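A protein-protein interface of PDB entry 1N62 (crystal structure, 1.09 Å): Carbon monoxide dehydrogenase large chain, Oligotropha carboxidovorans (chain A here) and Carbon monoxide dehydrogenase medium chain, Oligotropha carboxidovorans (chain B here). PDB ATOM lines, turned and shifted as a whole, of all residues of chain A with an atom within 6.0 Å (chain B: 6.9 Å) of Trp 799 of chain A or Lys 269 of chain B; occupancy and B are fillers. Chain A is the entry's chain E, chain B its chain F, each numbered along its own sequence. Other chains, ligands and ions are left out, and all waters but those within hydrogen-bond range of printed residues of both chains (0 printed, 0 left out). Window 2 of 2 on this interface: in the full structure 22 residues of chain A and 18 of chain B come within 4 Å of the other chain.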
ATOM      1  N   VAL A 670      10.222  31.321 -31.456  1.00  0.00           N
ATOM      2  CA  VAL A 670      10.861  30.060 -31.809  1.00  0.00           C
ATOM      3  C   VAL A 670      12.357  30.184 -31.937  1.00  0.00           C
ATOM      4  O   VAL A 670      13.029  29.173 -31.924  1.00  0.00           O
ATOM      5  CB  VAL A 670      10.290  29.470 -33.070  1.00  0.00           C
ATOM      6  CG1 VAL A 670       8.806  29.260 -32.910  1.00  0.00           C
ATOM      7  CG2 VAL A 670      10.630  30.337 -34.283  1.00  0.00           C
ATOM      8  N   ASP A 671      12.852  31.404 -32.114  1.00  0.00           N
ATOM      9  CA  ASP A 671      14.253  31.611 -32.349  1.00  0.00           C
ATOM     10  C   ASP A 671      15.046  31.563 -31.081  1.00  0.00           C
ATOM     11  O   ASP A 671      16.237  31.258 -31.136  1.00  0.00           O
ATOM     12  CB  ASP A 671      14.459  32.897 -33.099  1.00  0.00           C
ATOM     13  CG  ASP A 671      13.954  32.791 -34.502  1.00  0.00           C
ATOM     14  OD1 ASP A 671      14.143  31.709 -35.125  1.00  0.00           O
ATOM     15  OD2 ASP A 671      13.338  33.729 -35.038  1.00  0.00           O
ATOM     16  N   THR A 672      14.454  31.950 -29.974  1.00  0.00           N
ATOM     17  CA  THR A 672      15.133  31.880 -28.701  1.00  0.00           C
ATOM     18  C   THR A 672      14.606  30.777 -27.824  1.00  0.00           C
ATOM     19  O   THR A 672      15.243  30.444 -26.845  1.00  0.00           O
ATOM     20  CB  THR A 672      15.020  33.178 -27.939  1.00  0.00           C
ATOM     21  OG1 THR A 672      13.631  33.479 -27.777  1.00  0.00           O
ATOM     22  CG2 THR A 672      15.686  34.349 -28.706  1.00  0.00           C
ATOM     23  N   GLY A 673      13.407  30.311 -28.095  1.00  0.00           N
ATOM     24  CA  GLY A 673      12.731  29.407 -27.185  1.00  0.00           C
ATOM     25  C   GLY A 673      12.017  30.078 -26.061  1.00  0.00           C
ATOM     26  O   GLY A 673      11.454  29.382 -25.220  1.00  0.00           O
ATOM     27  N   TYR A 781       3.468  24.211 -30.656  1.00  0.00           N
ATOM     28  CA  TYR A 781       4.287  23.553 -31.646  1.00  0.00           C
ATOM     29  C   TYR A 781       3.573  22.429 -32.361  1.00  0.00           C
ATOM     30  O   TYR A 781       4.151  21.823 -33.260  1.00  0.00           O
ATOM     31  CB  TYR A 781       5.505  22.948 -30.999  1.00  0.00           C
ATOM     32  CG  TYR A 781       6.541  23.947 -30.624  1.00  0.00           C
ATOM     33  CD1 TYR A 781       7.519  24.323 -31.526  1.00  0.00           C
ATOM     34  CD2 TYR A 781       6.608  24.465 -29.336  1.00  0.00           C
ATOM     35  CE1 TYR A 781       8.476  25.217 -31.181  1.00  0.00           C
ATOM     36  CE2 TYR A 781       7.594  25.325 -28.988  1.00  0.00           C
ATOM     37  CZ  TYR A 781       8.516  25.719 -29.914  1.00  0.00           C
ATOM     38  OH  TYR A 781       9.459  26.617 -29.490  1.00  0.00           O
ATOM     39  N   ASP A 794      11.742  25.387 -20.782  1.00  0.00           N
ATOM     40  CA  ASP A 794      12.586  26.539 -20.725  1.00  0.00           C
ATOM     41  C   ASP A 794      13.160  26.826 -22.086  1.00  0.00           C
ATOM     42  O   ASP A 794      12.913  26.136 -23.057  1.00  0.00           O
ATOM     43  CB  ASP A 794      13.617  26.423 -19.643  1.00  0.00           C
ATOM     44  CG  ASP A 794      14.582  25.329 -19.857  1.00  0.00           C
ATOM     45  OD1 ASP A 794      14.466  24.565 -20.845  1.00  0.00           O
ATOM     46  OD2 ASP A 794      15.466  25.131 -18.980  1.00  0.00           O
ATOM     47  N   ALA A 795      13.888  27.910 -22.173  1.00  0.00           N
ATOM     48  CA  ALA A 795      14.176  28.446 -23.493  1.00  0.00           C
ATOM     49  C   ALA A 795      15.109  27.551 -24.265  1.00  0.00           C
ATOM     50  O   ALA A 795      14.888  27.331 -25.449  1.00  0.00           O
ATOM     51  CB  ALA A 795      14.719  29.828 -23.386  1.00  0.00           C
ATOM     52  N   TRP A 796      16.110  26.952 -23.628  1.00  0.00           N
ATOM     53  CA  TRP A 796      17.014  26.134 -24.403  1.00  0.00           C
ATOM     54  C   TRP A 796      16.287  24.928 -24.930  1.00  0.00           C
ATOM     55  O   TRP A 796      16.564  24.475 -26.029  1.00  0.00           O
ATOM     56  CB  TRP A 796      18.296  25.748 -23.663  1.00  0.00           C
ATOM     57  CG  TRP A 796      18.221  24.696 -22.626  1.00  0.00           C
ATOM     58  CD1 TRP A 796      18.115  24.902 -21.300  1.00  0.00           C
ATOM     59  CD2 TRP A 796      18.318  23.286 -22.801  1.00  0.00           C
ATOM     60  NE1 TRP A 796      18.199  23.717 -20.621  1.00  0.00           N
ATOM     61  CE2 TRP A 796      18.307  22.704 -21.523  1.00  0.00           C
ATOM     62  CE3 TRP A 796      18.485  22.453 -23.907  1.00  0.00           C
ATOM     63  CZ2 TRP A 796      18.451  21.343 -21.318  1.00  0.00           C
ATOM     64  CZ3 TRP A 796      18.589  21.109 -23.709  1.00  0.00           C
ATOM     65  CH2 TRP A 796      18.579  20.558 -22.421  1.00  0.00           C
ATOM     66  N   ARG A 797      15.427  24.356 -24.113  1.00  0.00           N
ATOM     67  CA  ARG A 797      14.716  23.195 -24.549  1.00  0.00           C
ATOM     68  C   ARG A 797      13.761  23.520 -25.655  1.00  0.00           C
ATOM     69  O   ARG A 797      13.629  22.729 -26.596  1.00  0.00           O
ATOM     70  CB  ARG A 797      14.062  22.478 -23.386  1.00  0.00           C
ATOM     71  CG  ARG A 797      15.047  21.476 -22.824  1.00  0.00           C
ATOM     72  CD  ARG A 797      14.677  20.905 -21.504  1.00  0.00           C
ATOM     73  NE  ARG A 797      15.048  21.831 -20.450  1.00  0.00           N
ATOM     74  CZ  ARG A 797      15.575  21.517 -19.291  1.00  0.00           C
ATOM     75  NH1 ARG A 797      15.813  20.268 -18.960  1.00  0.00           N
ATOM     76  NH2 ARG A 797      15.929  22.483 -18.477  1.00  0.00           N
ATOM     77  N   LEU A 798      13.089  24.662 -25.585  1.00  0.00           N
ATOM     78  CA  LEU A 798      12.204  25.005 -26.669  1.00  0.00           C
ATOM     79  C   LEU A 798      12.992  25.422 -27.887  1.00  0.00           C
ATOM     80  O   LEU A 798      12.572  25.172 -29.015  1.00  0.00           O
ATOM     81  CB  LEU A 798      11.187  26.065 -26.284  1.00  0.00           C
ATOM     82  CG  LEU A 798      10.257  25.627 -25.166  1.00  0.00           C
ATOM     83  CD1 LEU A 798       9.208  26.667 -25.040  1.00  0.00           C
ATOM     84  CD2 LEU A 798       9.681  24.251 -25.425  1.00  0.00           C
ATOM     85  N   TRP A 799      14.143  26.030 -27.713  1.00  0.00           N
ATOM     86  CA  TRP A 799      15.010  26.239 -28.851  1.00  0.00           C
ATOM     87  C   TRP A 799      15.357  24.934 -29.531  1.00  0.00           C
ATOM     88  O   TRP A 799      15.352  24.870 -30.751  1.00  0.00           O
ATOM     89  CB  TRP A 799      16.269  26.954 -28.413  1.00  0.00           C
ATOM     90  CG  TRP A 799      17.177  27.190 -29.569  1.00  0.00           C
ATOM     91  CD1 TRP A 799      17.181  28.269 -30.380  1.00  0.00           C
ATOM     92  CD2 TRP A 799      18.283  26.391 -29.963  1.00  0.00           C
ATOM     93  NE1 TRP A 799      18.172  28.157 -31.321  1.00  0.00           N
ATOM     94  CE2 TRP A 799      18.851  26.993 -31.096  1.00  0.00           C
ATOM     95  CE3 TRP A 799      18.835  25.205 -29.498  1.00  0.00           C
ATOM     96  CZ2 TRP A 799      19.954  26.472 -31.748  1.00  0.00           C
ATOM     97  CZ3 TRP A 799      19.890  24.648 -30.208  1.00  0.00           C
ATOM     98  CH2 TRP A 799      20.448  25.295 -31.292  1.00  0.00           C
ATOM     99  N   LYS A 800      15.697  23.922 -28.754  1.00  0.00           N
ATOM    100  CA  LYS A 800      16.049  22.630 -29.317  1.00  0.00           C
ATOM    101  C   LYS A 800      14.895  22.061 -30.097  1.00  0.00           C
ATOM    102  O   LYS A 800      15.083  21.478 -31.146  1.00  0.00           O
ATOM    103  CB  LYS A 800      16.447  21.644 -28.234  1.00  0.00           C
ATOM    104  CG  LYS A 800      17.804  21.861 -27.642  1.00  0.00           C
ATOM    105  CD  LYS A 800      18.861  21.338 -28.558  1.00  0.00           C
ATOM    106  CE  LYS A 800      20.239  21.617 -27.995  1.00  0.00           C
ATOM    107  NZ  LYS A 800      21.278  20.736 -28.560  1.00  0.00           N
ATOM    108  N   VAL A 801      13.676  22.246 -29.596  1.00  0.00           N
ATOM    109  CA  VAL A 801      12.513  21.783 -30.312  1.00  0.00           C
ATOM    110  C   VAL A 801      12.528  22.423 -31.687  1.00  0.00           C
ATOM    111  O   VAL A 801      12.413  21.755 -32.713  1.00  0.00           O
ATOM    112  CB  VAL A 801      11.234  22.115 -29.553  1.00  0.00           C
ATOM    113  CG1 VAL A 801      10.049  21.871 -30.436  1.00  0.00           C
ATOM    114  CG2 VAL A 801      11.133  21.285 -28.299  1.00  0.00           C
ATOM    115  N   GLY A 802      12.650  23.736 -31.741  1.00  0.00           N
ATOM    116  CA  GLY A 802      12.616  24.411 -33.010  1.00  0.00           C
ATOM    117  C   GLY A 802      13.810  24.091 -33.878  1.00  0.00           C
ATOM    118  O   GLY A 802      13.672  23.977 -35.092  1.00  0.00           O
ATOM    119  N   GLU A 803      14.960  23.878 -33.277  1.00  0.00           N
ATOM    120  CA  GLU A 803      16.147  23.539 -34.007  1.00  0.00           C
ATOM    121  C   GLU A 803      15.887  22.252 -34.748  1.00  0.00           C
ATOM    122  O   GLU A 803      16.161  22.150 -35.929  1.00  0.00           O
ATOM    123  CB  GLU A 803      17.300  23.373 -33.031  1.00  0.00           C
ATOM    124  CG  GLU A 803      18.623  23.069 -33.696  1.00  0.00           C
ATOM    125  CD  GLU A 803      19.096  24.128 -34.685  1.00  0.00           C
ATOM    126  OE1 GLU A 803      18.760  25.333 -34.553  1.00  0.00           O
ATOM    127  OE2 GLU A 803      19.882  23.737 -35.581  1.00  0.00           O
ATOM    128  N   GLN A 804      15.341  21.285 -34.022  1.00  0.00           N
ATOM    129  CA  GLN A 804      15.109  19.966 -34.550  1.00  0.00           C
ATOM    130  C   GLN A 804      13.934  19.937 -35.521  1.00  0.00           C
ATOM    131  O   GLN A 804      13.895  19.093 -36.402  1.00  0.00           O
ATOM    132  CB  GLN A 804      14.854  19.026 -33.381  1.00  0.00           C
ATOM    133  CG  GLN A 804      16.131  18.783 -32.644  1.00  0.00           C
ATOM    134  CD  GLN A 804      15.954  18.349 -31.225  1.00  0.00           C
ATOM    135  OE1 GLN A 804      16.920  18.362 -30.455  1.00  0.00           O
ATOM    136  NE2 GLN A 804      14.772  17.843 -30.895  1.00  0.00           N
ATOM    137  N   HIS A 808      15.254  27.160 -37.716  1.00  0.00           N
ATOM    138  CA  HIS A 808      16.270  28.169 -37.565  1.00  0.00           C
ATOM    139  C   HIS A 808      17.114  28.368 -38.813  1.00  0.00           C
ATOM    140  O   HIS A 808      18.163  28.970 -38.753  1.00  0.00           O
ATOM    141  CB  HIS A 808      17.146  27.838 -36.388  1.00  0.00           C
ATOM    142  CG  HIS A 808      16.390  27.784 -35.109  1.00  0.00           C
ATOM    143  ND1 HIS A 808      16.703  26.890 -34.111  1.00  0.00           N
ATOM    144  CD2 HIS A 808      15.342  28.516 -34.668  1.00  0.00           C
ATOM    145  CE1 HIS A 808      15.867  27.071 -33.107  1.00  0.00           C
ATOM    146  NE2 HIS A 808      15.037  28.046 -33.426  1.00  0.00           N
ATOM    147  N   ALA B 196      23.208  34.332 -22.958  1.00  0.00           N
ATOM    148  CA  ALA B 196      24.098  35.066 -23.845  1.00  0.00           C
ATOM    149  C   ALA B 196      23.647  36.513 -23.775  1.00  0.00           C
ATOM    150  O   ALA B 196      22.455  36.794 -23.530  1.00  0.00           O
ATOM    151  CB  ALA B 196      23.951  34.558 -25.248  1.00  0.00           C
ATOM    152  N   VAL B 247      26.846  38.089 -37.337  1.00  0.00           N
ATOM    153  CA  VAL B 247      26.491  36.967 -36.511  1.00  0.00           C
ATOM    154  C   VAL B 247      27.473  35.825 -36.696  1.00  0.00           C
ATOM    155  O   VAL B 247      27.877  35.187 -35.748  1.00  0.00           O
ATOM    156  CB  VAL B 247      25.074  36.522 -36.787  1.00  0.00           C
ATOM    157  CG1 VAL B 247      24.808  35.143 -36.220  1.00  0.00           C
ATOM    158  CG2 VAL B 247      24.097  37.545 -36.229  1.00  0.00           C
ATOM    159  N   GLU B 251      29.479  34.428 -33.621  1.00  0.00           N
ATOM    160  CA  GLU B 251      29.339  33.056 -33.179  1.00  0.00           C
ATOM    161  C   GLU B 251      30.664  32.333 -33.192  1.00  0.00           C
ATOM    162  O   GLU B 251      30.937  31.475 -32.361  1.00  0.00           O
ATOM    163  CB  GLU B 251      28.365  32.326 -34.063  1.00  0.00           C
ATOM    164  CG  GLU B 251      26.951  32.775 -33.834  1.00  0.00           C
ATOM    165  CD  GLU B 251      25.999  32.144 -34.805  1.00  0.00           C
ATOM    166  OE1 GLU B 251      26.472  31.579 -35.839  1.00  0.00           O
ATOM    167  OE2 GLU B 251      24.783  32.276 -34.595  1.00  0.00           O
ATOM    168  N   THR B 254      32.702  32.330 -30.104  1.00  0.00           N
ATOM    169  CA  THR B 254      32.158  31.870 -28.855  1.00  0.00           C
ATOM    170  C   THR B 254      32.708  30.499 -28.503  1.00  0.00           C
ATOM    171  O   THR B 254      33.009  29.716 -29.394  1.00  0.00           O
ATOM    172  CB  THR B 254      30.654  31.875 -28.863  1.00  0.00           C
ATOM    173  OG1 THR B 254      30.149  30.926 -29.796  1.00  0.00           O
ATOM    174  CG2 THR B 254      30.098  33.213 -29.221  1.00  0.00           C
ATOM    175  N   PRO B 256      30.873  28.595 -25.448  1.00  0.00           N
ATOM    176  CA  PRO B 256      30.117  28.706 -24.202  1.00  0.00           C
ATOM    177  C   PRO B 256      30.175  27.444 -23.380  1.00  0.00           C
ATOM    178  O   PRO B 256      30.547  26.371 -23.837  1.00  0.00           O
ATOM    179  CB  PRO B 256      28.683  28.922 -24.682  1.00  0.00           C
ATOM    180  CG  PRO B 256      28.817  29.364 -26.078  1.00  0.00           C
ATOM    181  CD  PRO B 256      30.004  28.668 -26.625  1.00  0.00           C
ATOM    182  N   PRO B 263      22.984  24.126 -23.567  1.00  0.00           N
ATOM    183  CA  PRO B 263      24.231  23.612 -24.107  1.00  0.00           C
ATOM    184  C   PRO B 263      24.903  24.633 -24.972  1.00  0.00           C
ATOM    185  O   PRO B 263      24.329  25.648 -25.390  1.00  0.00           O
ATOM    186  CB  PRO B 263      23.770  22.431 -24.963  1.00  0.00           C
ATOM    187  CG  PRO B 263      22.449  22.864 -25.450  1.00  0.00           C
ATOM    188  CD  PRO B 263      21.817  23.635 -24.311  1.00  0.00           C
ATOM    189  N   ALA B 264      26.193  24.414 -25.136  1.00  0.00           N
ATOM    190  CA  ALA B 264      27.016  25.379 -25.820  1.00  0.00           C
ATOM    191  C   ALA B 264      26.464  25.816 -27.165  1.00  0.00           C
ATOM    192  O   ALA B 264      26.492  26.992 -27.492  1.00  0.00           O
ATOM    193  CB  ALA B 264      28.380  24.811 -26.033  1.00  0.00           C
ATOM    194  N   GLU B 265      25.918  24.887 -27.937  1.00  0.00           N
ATOM    195  CA  GLU B 265      25.433  25.247 -29.243  1.00  0.00           C
ATOM    196  C   GLU B 265      24.253  26.206 -29.203  1.00  0.00           C
ATOM    197  O   GLU B 265      24.152  27.121 -30.013  1.00  0.00           O
ATOM    198  CB  GLU B 265      25.050  23.988 -30.014  1.00  0.00           C
ATOM    199  CG  GLU B 265      23.984  23.101 -29.374  1.00  0.00           C
ATOM    200  CD  GLU B 265      24.524  22.132 -28.327  1.00  0.00           C
ATOM    201  OE1 GLU B 265      25.745  22.190 -28.031  1.00  0.00           O
ATOM    202  OE2 GLU B 265      23.786  21.159 -27.999  1.00  0.00           O
ATOM    203  N   TYR B 266      23.429  26.083 -28.176  1.00  0.00           N
ATOM    204  CA  TYR B 266      22.333  26.999 -28.034  1.00  0.00           C
ATOM    205  C   TYR B 266      22.883  28.365 -27.718  1.00  0.00           C
ATOM    206  O   TYR B 266      22.426  29.380 -28.207  1.00  0.00           O
ATOM    207  CB  TYR B 266      21.437  26.534 -26.878  1.00  0.00           C
ATOM    208  CG  TYR B 266      20.391  27.523 -26.469  1.00  0.00           C
ATOM    209  CD1 TYR B 266      19.484  27.994 -27.371  1.00  0.00           C
ATOM    210  CD2 TYR B 266      20.322  28.013 -25.173  1.00  0.00           C
ATOM    211  CE1 TYR B 266      18.479  28.851 -26.984  1.00  0.00           C
ATOM    212  CE2 TYR B 266      19.334  28.894 -24.787  1.00  0.00           C
ATOM    213  CZ  TYR B 266      18.415  29.312 -25.694  1.00  0.00           C
ATOM    214  OH  TYR B 266      17.408  30.145 -25.280  1.00  0.00           O
ATOM    215  N   ARG B 267      23.797  28.386 -26.783  1.00  0.00           N
ATOM    216  CA  ARG B 267      24.286  29.663 -26.324  1.00  0.00           C
ATOM    217  C   ARG B 267      25.040  30.414 -27.420  1.00  0.00           C
ATOM    218  O   ARG B 267      24.954  31.631 -27.496  1.00  0.00           O
ATOM    219  CB  ARG B 267      25.136  29.462 -25.085  1.00  0.00           C
ATOM    220  CG  ARG B 267      24.295  28.838 -23.982  1.00  0.00           C
ATOM    221  CD  ARG B 267      25.022  28.608 -22.710  1.00  0.00           C
ATOM    222  NE  ARG B 267      25.359  29.847 -22.076  1.00  0.00           N
ATOM    223  CZ  ARG B 267      25.894  29.893 -20.887  1.00  0.00           C
ATOM    224  NH1 ARG B 267      26.390  28.807 -20.336  1.00  0.00           N
ATOM    225  NH2 ARG B 267      25.957  31.024 -20.248  1.00  0.00           N
ATOM    226  N   THR B 268      25.758  29.681 -28.261  1.00  0.00           N
ATOM    227  CA  THR B 268      26.376  30.271 -29.413  1.00  0.00           C
ATOM    228  C   THR B 268      25.331  30.940 -30.286  1.00  0.00           C
ATOM    229  O   THR B 268      25.477  32.103 -30.693  1.00  0.00           O
ATOM    230  CB  THR B 268      27.176  29.234 -30.163  1.00  0.00           C
ATOM    231  OG1 THR B 268      28.343  28.935 -29.395  1.00  0.00           O
ATOM    232  CG2 THR B 268      27.635  29.742 -31.525  1.00  0.00           C
ATOM    233  N   LYS B 269      24.261  30.221 -30.576  1.00  0.00           N
ATOM    234  CA  LYS B 269      23.236  30.812 -31.390  1.00  0.00           C
ATOM    235  C   LYS B 269      22.597  32.007 -30.705  1.00  0.00           C
ATOM    236  O   LYS B 269      22.271  33.000 -31.341  1.00  0.00           O
ATOM    237  CB  LYS B 269      22.194  29.767 -31.751  1.00  0.00           C
ATOM    238  CG  LYS B 269      22.678  28.715 -32.750  1.00  0.00           C
ATOM    239  CD  LYS B 269      23.391  29.279 -33.989  1.00  0.00           C
ATOM    240  CE  LYS B 269      22.476  30.055 -34.914  1.00  0.00           C
ATOM    241  NZ  LYS B 269      23.291  30.585 -36.082  1.00  0.00           N
ATOM    242  N   MET B 270      22.475  31.943 -29.384  1.00  0.00           N
ATOM    243  CA  MET B 270      21.838  33.040 -28.678  1.00  0.00           C
ATOM    244  C   MET B 270      22.738  34.244 -28.639  1.00  0.00           C
ATOM    245  O   MET B 270      22.233  35.365 -28.689  1.00  0.00           O
ATOM    246  CB  MET B 270      21.438  32.651 -27.269  1.00  0.00           C
ATOM    247  CG  MET B 270      20.326  31.637 -27.229  1.00  0.00           C
ATOM    248  SD  MET B 270      18.872  32.126 -28.182  1.00  0.00           S
ATOM    249  CE  MET B 270      19.166  31.269 -29.736  1.00  0.00           C
ATOM    250  N   ALA B 271      24.051  34.032 -28.683  1.00  0.00           N
ATOM    251  CA  ALA B 271      24.933  35.165 -28.838  1.00  0.00           C
ATOM    252  C   ALA B 271      24.595  35.882 -30.145  1.00  0.00           C
ATOM    253  O   ALA B 271      24.552  37.107 -30.213  1.00  0.00           O
ATOM    254  CB  ALA B 271      26.354  34.726 -28.825  1.00  0.00           C
ATOM    255  N   GLY B 272      24.411  35.107 -31.202  1.00  0.00           N
ATOM    256  CA  GLY B 272      24.037  35.679 -32.474  1.00  0.00           C
ATOM    257  C   GLY B 272      22.704  36.415 -32.439  1.00  0.00           C
ATOM    258  O   GLY B 272      22.539  37.496 -33.015  1.00  0.00           O
ATOM    259  N   VAL B 273      21.713  35.807 -31.813  1.00  0.00           N
ATOM    260  CA  VAL B 273      20.408  36.434 -31.785  1.00  0.00           C
ATOM    261  C   VAL B 273      20.453  37.709 -30.958  1.00  0.00           C
ATOM    262  O   VAL B 273      19.857  38.719 -31.314  1.00  0.00           O
ATOM    263  CB  VAL B 273      19.341  35.482 -31.247  1.00  0.00           C
ATOM    264  CG1 VAL B 273      18.014  36.206 -31.120  1.00  0.00           C
ATOM    265  CG2 VAL B 273      19.262  34.282 -32.131  1.00  0.00           C
ATOM    266  N   MET B 274      21.117  37.650 -29.819  1.00  0.00           N
ATOM    267  CA  MET B 274      21.221  38.851 -29.019  1.00  0.00           C
ATOM    268  C   MET B 274      21.934  39.930 -29.806  1.00  0.00           C
ATOM    269  O   MET B 274      21.577  41.096 -29.726  1.00  0.00           O
ATOM    270  CB  MET B 274      21.913  38.561 -27.696  1.00  0.00           C
ATOM    271  CG  MET B 274      21.139  37.674 -26.734  1.00  0.00           C
ATOM    272  SD  MET B 274      19.497  38.263 -26.351  1.00  0.00           S
ATOM    273  CE  MET B 274      18.511  37.300 -27.389  1.00  0.00           C
ATOM    274  N   LEU B 275      22.983  39.541 -30.518  1.00  0.00           N
ATOM    275  CA  LEU B 275      23.682  40.481 -31.353  1.00  0.00           C
ATOM    276  C   LEU B 275      22.728  41.128 -32.325  1.00  0.00           C
ATOM    277  O   LEU B 275      22.727  42.339 -32.497  1.00  0.00           O
ATOM    278  CB  LEU B 275      24.846  39.793 -32.041  1.00  0.00           C
ATOM    279  CG  LEU B 275      25.676  40.708 -32.931  1.00  0.00           C
ATOM    280  CD1 LEU B 275      25.996  41.967 -32.189  1.00  0.00           C
ATOM    281  CD2 LEU B 275      26.910  39.935 -33.346  1.00  0.00           C
ATOM    282  N   ARG B 276      22.015  40.310 -33.083  1.00  0.00           N
ATOM    283  CA  ARG B 276      21.107  40.868 -34.070  1.00  0.00           C
ATOM    284  C   ARG B 276      20.173  41.867 -33.428  1.00  0.00           C
ATOM    285  O   ARG B 276      19.930  42.931 -33.987  1.00  0.00           O
ATOM    286  CB  ARG B 276      20.238  39.805 -34.646  1.00  0.00           C
ATOM    287  CG  ARG B 276      20.829  38.995 -35.670  1.00  0.00           C
ATOM    288  CD  ARG B 276      19.815  38.121 -36.308  1.00  0.00           C
ATOM    289  NE  ARG B 276      20.451  37.012 -36.966  1.00  0.00           N
ATOM    290  CZ  ARG B 276      20.901  37.088 -38.186  1.00  0.00           C
ATOM    291  NH1 ARG B 276      20.724  38.218 -38.869  1.00  0.00           N
ATOM    292  NH2 ARG B 276      21.586  36.085 -38.711  1.00  0.00           N
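The side-chain amino group (NZ) of Lys 800 of chain A lies within salt-bridge range of the side-chain carboxylate (OE2) of Glu 265 of chain B. The backbone carbonyl oxygen of Thr 672 of chain A is in hydrogen-bond range of the side-chain hydroxyl of Tyr 266 of chain B (2.7 Å).
OE2 of Glu 251 of chain B lies within salt-bridge range of NZ of Lys 269 of chain B (2.7 Å). NE1 of Trp 796 of chain A is in hydrogen-bond range of OD2 of Asp 794 of chain A, 3.5 Å away. NE1 of Trp 799 of chain A lies close to ND1 of His 808 of chain A (3.4 Å).
Among the printed residues, pairs that only touch across the chains: Asp 671 of chain A with Met 270 of chain B, Thr 672 of chain A with Met 270 of chain B, Thr 672 of chain A with Val 273 of chain B, Ala 795 of chain A with Tyr 266 of chain B, Trp 796 of chain A with Pro 263 of chain B, Trp 796 of chain A with Tyr 266 of chain B, Trp 799 of chain A with Tyr 266 of chain B, Trp 799 of chain A with Lys 269 of chain B, Trp 799 of chain A with Met 270 of chain B and Lys 800 of chain A with Pro 263 of chain B.
Of the printed residues of chain B, Ala 795 of chain A touches Tyr 266. Printed residues of chain B within 4 Å of Lys 800 of chain A: Pro 263 (3.6 Å) and Glu 265 (2.6 Å). Gln 804 of chain A touches none of the printed residues of chain B. Glu 251 of chain B touches none of the printed residues of chain A. Lys 269 of chain B touches just one residue of chain A: Trp 799. The nearest residue of chain B that does not touch Trp 799 of chain A is Glu 265 of chain B (4.3 Å). The nearest printed residue of chain B that does not touch Thr 672 of chain A is Met 274 of chain B (4.3 Å).
Hydrophobic or aromatic side chains of chain B within 4 Å of the printed part of chain A: Pro 263, Tyr 266, Met 270 and Val 273. Of the 17 printed residues of chain A, 6 touch a printed residue of chain B. Printed residues of chain A that touch a printed residue of chain B: Asp 671, Thr 672, Ala 795, Trp 796, Trp 799 and Lys 800. Among the printed residues, 12 pairs touch across the chains. Among the printed residues, Asp or Glu carboxylates within 4 Å of a Lys or Arg side-chain nitrogen of the other chain: Lys 800 of chain A with Glu 265 of chain B (2.6 Å).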
